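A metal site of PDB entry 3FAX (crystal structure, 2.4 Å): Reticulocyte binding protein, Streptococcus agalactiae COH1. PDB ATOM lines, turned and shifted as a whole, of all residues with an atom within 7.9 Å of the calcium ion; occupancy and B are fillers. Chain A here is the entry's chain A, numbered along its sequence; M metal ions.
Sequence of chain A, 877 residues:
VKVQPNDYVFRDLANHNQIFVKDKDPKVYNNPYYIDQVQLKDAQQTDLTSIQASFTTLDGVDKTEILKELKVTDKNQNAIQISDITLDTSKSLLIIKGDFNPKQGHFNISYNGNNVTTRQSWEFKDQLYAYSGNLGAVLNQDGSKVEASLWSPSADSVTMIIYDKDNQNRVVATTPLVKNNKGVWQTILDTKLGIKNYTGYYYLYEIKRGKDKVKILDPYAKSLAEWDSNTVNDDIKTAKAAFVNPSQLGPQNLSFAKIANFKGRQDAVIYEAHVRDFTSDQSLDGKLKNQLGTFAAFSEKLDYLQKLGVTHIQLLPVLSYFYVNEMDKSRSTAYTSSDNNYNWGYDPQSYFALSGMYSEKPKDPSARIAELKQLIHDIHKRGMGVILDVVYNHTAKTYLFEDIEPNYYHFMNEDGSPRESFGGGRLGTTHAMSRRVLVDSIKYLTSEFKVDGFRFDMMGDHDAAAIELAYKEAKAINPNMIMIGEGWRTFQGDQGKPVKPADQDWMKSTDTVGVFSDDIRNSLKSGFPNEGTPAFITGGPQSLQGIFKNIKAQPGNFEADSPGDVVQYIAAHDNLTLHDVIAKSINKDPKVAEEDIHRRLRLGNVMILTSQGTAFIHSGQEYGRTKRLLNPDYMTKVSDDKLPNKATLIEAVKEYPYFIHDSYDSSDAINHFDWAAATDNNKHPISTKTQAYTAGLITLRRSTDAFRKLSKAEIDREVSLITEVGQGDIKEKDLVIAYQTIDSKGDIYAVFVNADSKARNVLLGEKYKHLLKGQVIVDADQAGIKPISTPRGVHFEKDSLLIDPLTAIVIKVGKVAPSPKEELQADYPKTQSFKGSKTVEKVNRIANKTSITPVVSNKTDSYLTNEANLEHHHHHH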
ATOM      1  N   TYR A 321      18.985  -9.632  24.194  1.00  0.00           N
ATOM      2  CA  TYR A 321      20.259  -9.080  23.752  1.00  0.00           C
ATOM      3  C   TYR A 321      20.516  -9.454  22.290  1.00  0.00           C
ATOM      4  O   TYR A 321      19.983 -10.445  21.801  1.00  0.00           O
ATOM      5  CB  TYR A 321      21.423  -9.568  24.632  1.00  0.00           C
ATOM      6  CG  TYR A 321      21.445 -11.052  24.949  1.00  0.00           C
ATOM      7  CD1 TYR A 321      22.046 -11.968  24.089  1.00  0.00           C
ATOM      8  CD2 TYR A 321      20.903 -11.523  26.145  1.00  0.00           C
ATOM      9  CE1 TYR A 321      22.089 -13.320  24.387  1.00  0.00           C
ATOM     10  CE2 TYR A 321      20.940 -12.880  26.448  1.00  0.00           C
ATOM     11  CZ  TYR A 321      21.540 -13.768  25.577  1.00  0.00           C
ATOM     12  OH  TYR A 321      21.577 -15.125  25.881  1.00  0.00           O
ATOM     13  N   TYR A 323      23.460  -9.983  19.915  1.00  0.00           N
ATOM     14  CA  TYR A 323      24.339 -10.932  19.212  1.00  0.00           C
ATOM     15  C   TYR A 323      24.115 -12.405  19.593  1.00  0.00           C
ATOM     16  O   TYR A 323      24.803 -12.939  20.460  1.00  0.00           O
ATOM     17  CB  TYR A 323      25.821 -10.540  19.394  1.00  0.00           C
ATOM     18  CG  TYR A 323      26.212  -9.388  18.512  1.00  0.00           C
ATOM     19  CD1 TYR A 323      26.510  -8.134  19.054  1.00  0.00           C
ATOM     20  CD2 TYR A 323      26.279  -9.534  17.139  1.00  0.00           C
ATOM     21  CE1 TYR A 323      26.864  -7.073  18.242  1.00  0.00           C
ATOM     22  CE2 TYR A 323      26.629  -8.481  16.316  1.00  0.00           C
ATOM     23  CZ  TYR A 323      26.920  -7.261  16.874  1.00  0.00           C
ATOM     24  OH  TYR A 323      27.274  -6.222  16.059  1.00  0.00           O
ATOM     25  N   VAL A 324      23.155 -13.043  18.918  1.00  0.00           N
ATOM     26  CA  VAL A 324      22.800 -14.423  19.199  1.00  0.00           C
ATOM     27  C   VAL A 324      22.011 -15.073  18.083  1.00  0.00           C
ATOM     28  O   VAL A 324      21.377 -14.398  17.277  1.00  0.00           O
ATOM     29  CB  VAL A 324      21.914 -14.551  20.465  1.00  0.00           C
ATOM     30  CG1 VAL A 324      22.769 -14.810  21.665  1.00  0.00           C
ATOM     31  CG2 VAL A 324      21.017 -13.314  20.638  1.00  0.00           C
ATOM     32  N   SER A 338      36.326 -16.636  22.072  1.00  0.00           N
ATOM     33  CA  SER A 338      35.846 -15.795  20.976  1.00  0.00           C
ATOM     34  C   SER A 338      34.853 -16.564  20.135  1.00  0.00           C
ATOM     35  O   SER A 338      34.826 -17.802  20.161  1.00  0.00           O
ATOM     36  CB  SER A 338      37.014 -15.366  20.072  1.00  0.00           C
ATOM     37  OG  SER A 338      37.793 -14.341  20.674  1.00  0.00           O
ATOM     38  N   ASP A 339      34.023 -15.825  19.390  1.00  0.00           N
ATOM     39  CA  ASP A 339      33.142 -16.396  18.360  1.00  0.00           C
ATOM     40  C   ASP A 339      32.363 -17.605  18.871  1.00  0.00           C
ATOM     41  O   ASP A 339      32.444 -18.711  18.323  1.00  0.00           O
ATOM     42  CB  ASP A 339      33.961 -16.750  17.106  1.00  0.00           C
ATOM     43  CG  ASP A 339      34.660 -15.543  16.490  1.00  0.00           C
ATOM     44  OD1 ASP A 339      34.007 -14.492  16.327  1.00  0.00           O
ATOM     45  OD2 ASP A 339      35.861 -15.655  16.172  1.00  0.00           O
ATOM     46  N   ASN A 340      31.625 -17.389  19.959  1.00  0.00           N
ATOM     47  CA  ASN A 340      30.706 -18.374  20.507  1.00  0.00           C
ATOM     48  C   ASN A 340      29.301 -17.773  20.589  1.00  0.00           C
ATOM     49  O   ASN A 340      29.142 -16.610  20.981  1.00  0.00           O
ATOM     50  CB  ASN A 340      31.140 -18.818  21.908  1.00  0.00           C
ATOM     51  CG  ASN A 340      32.314 -19.789  21.873  1.00  0.00           C
ATOM     52  OD1 ASN A 340      32.132 -20.989  21.675  1.00  0.00           O
ATOM     53  ND2 ASN A 340      33.516 -19.277  22.107  1.00  0.00           N
ATOM     54  N   ASN A 341      28.300 -18.564  20.236  1.00  0.00           N
ATOM     55  CA  ASN A 341      26.903 -18.133  20.319  1.00  0.00           C
ATOM     56  C   ASN A 341      26.519 -17.796  21.762  1.00  0.00           C
ATOM     57  O   ASN A 341      25.507 -17.123  22.013  1.00  0.00           O
ATOM     58  CB  ASN A 341      25.959 -19.186  19.751  1.00  0.00           C
ATOM     59  CG  ASN A 341      24.580 -18.634  19.461  1.00  0.00           C
ATOM     60  OD1 ASN A 341      24.433 -17.623  18.774  1.00  0.00           O
ATOM     61  ND2 ASN A 341      23.554 -19.287  19.985  1.00  0.00           N
ATOM     62  N   TYR A 342      27.318 -18.280  22.708  1.00  0.00           N
ATOM     63  CA  TYR A 342      27.241 -17.837  24.083  1.00  0.00           C
ATOM     64  C   TYR A 342      27.333 -16.314  24.166  1.00  0.00           C
ATOM     65  O   TYR A 342      28.095 -15.675  23.423  1.00  0.00           O
ATOM     66  CB  TYR A 342      28.357 -18.467  24.910  1.00  0.00           C
ATOM     67  CG  TYR A 342      28.238 -18.183  26.394  1.00  0.00           C
ATOM     68  CD1 TYR A 342      27.463 -18.991  27.217  1.00  0.00           C
ATOM     69  CD2 TYR A 342      28.902 -17.090  26.962  1.00  0.00           C
ATOM     70  CE1 TYR A 342      27.363 -18.735  28.579  1.00  0.00           C
ATOM     71  CE2 TYR A 342      28.802 -16.828  28.311  1.00  0.00           C
ATOM     72  CZ  TYR A 342      28.032 -17.648  29.113  1.00  0.00           C
ATOM     73  OH  TYR A 342      27.922 -17.377  30.459  1.00  0.00           O
ATOM     74  N   ASN A 343      26.563 -15.752  25.085  1.00  0.00           N
ATOM     75  CA  ASN A 343      26.580 -14.327  25.346  1.00  0.00           C
ATOM     76  C   ASN A 343      26.086 -14.090  26.772  1.00  0.00           C
ATOM     77  O   ASN A 343      25.058 -14.633  27.183  1.00  0.00           O
ATOM     78  CB  ASN A 343      25.684 -13.631  24.321  1.00  0.00           C
ATOM     79  CG  ASN A 343      25.828 -12.132  24.321  1.00  0.00           C
ATOM     80  OD1 ASN A 343      26.358 -11.528  25.265  1.00  0.00           O
ATOM     81  ND2 ASN A 343      25.335 -11.502  23.270  1.00  0.00           N
ATOM     82  N   TRP A 344      26.858 -13.306  27.538  1.00  0.00           N
ATOM     83  CA  TRP A 344      26.446 -12.872  28.878  1.00  0.00           C
ATOM     84  C   TRP A 344      25.141 -12.073  28.812  1.00  0.00           C
ATOM     85  O   TRP A 344      24.257 -12.227  29.663  1.00  0.00           O
ATOM     86  CB  TRP A 344      27.527 -12.002  29.543  1.00  0.00           C
ATOM     87  CG  TRP A 344      28.607 -12.752  30.279  1.00  0.00           C
ATOM     88  CD1 TRP A 344      28.583 -14.065  30.690  1.00  0.00           C
ATOM     89  CD2 TRP A 344      29.860 -12.226  30.719  1.00  0.00           C
ATOM     90  NE1 TRP A 344      29.743 -14.377  31.340  1.00  0.00           N
ATOM     91  CE2 TRP A 344      30.555 -13.267  31.365  1.00  0.00           C
ATOM     92  CE3 TRP A 344      30.477 -10.975  30.615  1.00  0.00           C
ATOM     93  CZ2 TRP A 344      31.821 -13.098  31.908  1.00  0.00           C
ATOM     94  CZ3 TRP A 344      31.736 -10.810  31.164  1.00  0.00           C
ATOM     95  CH2 TRP A 344      32.390 -11.858  31.794  1.00  0.00           C
ATOM     96  N   ASP A 347      24.705  -6.661  25.602  1.00  0.00           N
ATOM     97  CA  ASP A 347      24.463  -5.819  24.410  1.00  0.00           C
ATOM     98  C   ASP A 347      22.943  -5.737  24.179  1.00  0.00           C
ATOM     99  O   ASP A 347      22.392  -6.473  23.354  1.00  0.00           O
ATOM    100  CB  ASP A 347      25.238  -6.321  23.168  1.00  0.00           C
ATOM    101  CG  ASP A 347      24.938  -7.764  22.805  1.00  0.00           C
ATOM    102  OD1 ASP A 347      25.161  -8.656  23.643  1.00  0.00           O
ATOM    103  OD2 ASP A 347      24.505  -7.992  21.653  1.00  0.00           O
ATOM    104  N   SER A 663      34.822 -13.803  30.079  1.00  0.00           N
ATOM    105  CA  SER A 663      34.253 -14.946  29.367  1.00  0.00           C
ATOM    106  C   SER A 663      32.899 -14.670  28.696  1.00  0.00           C
ATOM    107  O   SER A 663      32.123 -15.596  28.456  1.00  0.00           O
ATOM    108  CB  SER A 663      34.148 -16.154  30.311  1.00  0.00           C
ATOM    109  OG  SER A 663      33.319 -15.895  31.438  1.00  0.00           O
ATOM    110  N   TYR A 664      32.635 -13.409  28.352  1.00  0.00           N
ATOM    111  CA  TYR A 664      31.380 -13.029  27.707  1.00  0.00           C
ATOM    112  C   TYR A 664      31.158 -13.740  26.358  1.00  0.00           C
ATOM    113  O   TYR A 664      30.022 -14.070  26.008  1.00  0.00           O
ATOM    114  CB  TYR A 664      31.310 -11.503  27.512  1.00  0.00           C
ATOM    115  CG  TYR A 664      32.077 -10.968  26.326  1.00  0.00           C
ATOM    116  CD1 TYR A 664      31.420 -10.546  25.174  1.00  0.00           C
ATOM    117  CD2 TYR A 664      33.471 -10.869  26.350  1.00  0.00           C
ATOM    118  CE1 TYR A 664      32.114 -10.041  24.072  1.00  0.00           C
ATOM    119  CE2 TYR A 664      34.186 -10.361  25.255  1.00  0.00           C
ATOM    120  CZ  TYR A 664      33.496  -9.958  24.119  1.00  0.00           C
ATOM    121  OH  TYR A 664      34.174  -9.455  23.033  1.00  0.00           O
ATOM    122  N   ASP A 665      32.262 -13.993  25.624  1.00  0.00           N
ATOM    123  CA  ASP A 665      32.227 -14.614  24.298  1.00  0.00           C
ATOM    124  C   ASP A 665      32.883 -16.006  24.276  1.00  0.00           C
ATOM    125  O   ASP A 665      33.328 -16.483  23.225  1.00  0.00           O
ATOM    126  CB  ASP A 665      32.933 -13.696  23.288  1.00  0.00           C
ATOM    127  CG  ASP A 665      32.465 -13.901  21.860  1.00  0.00           C
ATOM    128  OD1 ASP A 665      31.452 -14.620  21.640  1.00  0.00           O
ATOM    129  OD2 ASP A 665      33.090 -13.325  20.948  1.00  0.00           O
ATOM    130  N   SER A 666      32.949 -16.655  25.441  1.00  0.00           N
ATOM    131  CA  SER A 666      33.636 -17.935  25.600  1.00  0.00           C
ATOM    132  C   SER A 666      32.644 -19.078  25.537  1.00  0.00           C
ATOM    133  O   SER A 666      31.444 -18.881  25.723  1.00  0.00           O
ATOM    134  CB  SER A 666      34.393 -17.962  26.925  1.00  0.00           C
ATOM    135  OG  SER A 666      35.338 -16.908  26.996  1.00  0.00           O
HETATM  136 CA    CA M   1      28.937 -14.344  21.630  1.00  0.00          CA
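ND2 of Asn 340 lies within hydrogen-bond range of O of Ser 338.
The backbone NH (N) of Asp 339 is in hydrogen-bond range of the side-chain carboxylate (OD2) of Asp 665 (3.1 Å).
N of Ser 338 lies within hydrogen-bond range of O of Asp 665, at 3.2 Å.
The calcium ion is bound by the backbone carbonyl oxygen of Asn 340 (2.4 Å), the backbone carbonyl oxygen of Tyr 342 (2.4 Å) and the side-chain carboxylate of Asp 665 (2.5 Å).
The calcium ion has three donor atoms within binding distance.
Within 4 Å of the calcium ion: Asn 340, Tyr 342 and Asp 665.
Along chain A the residues within 4 Å of the calcium ion span positions 340 to 665.
The nearest printed residue that does not touch the calcium ion is Asn 341 (4.2 Å).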
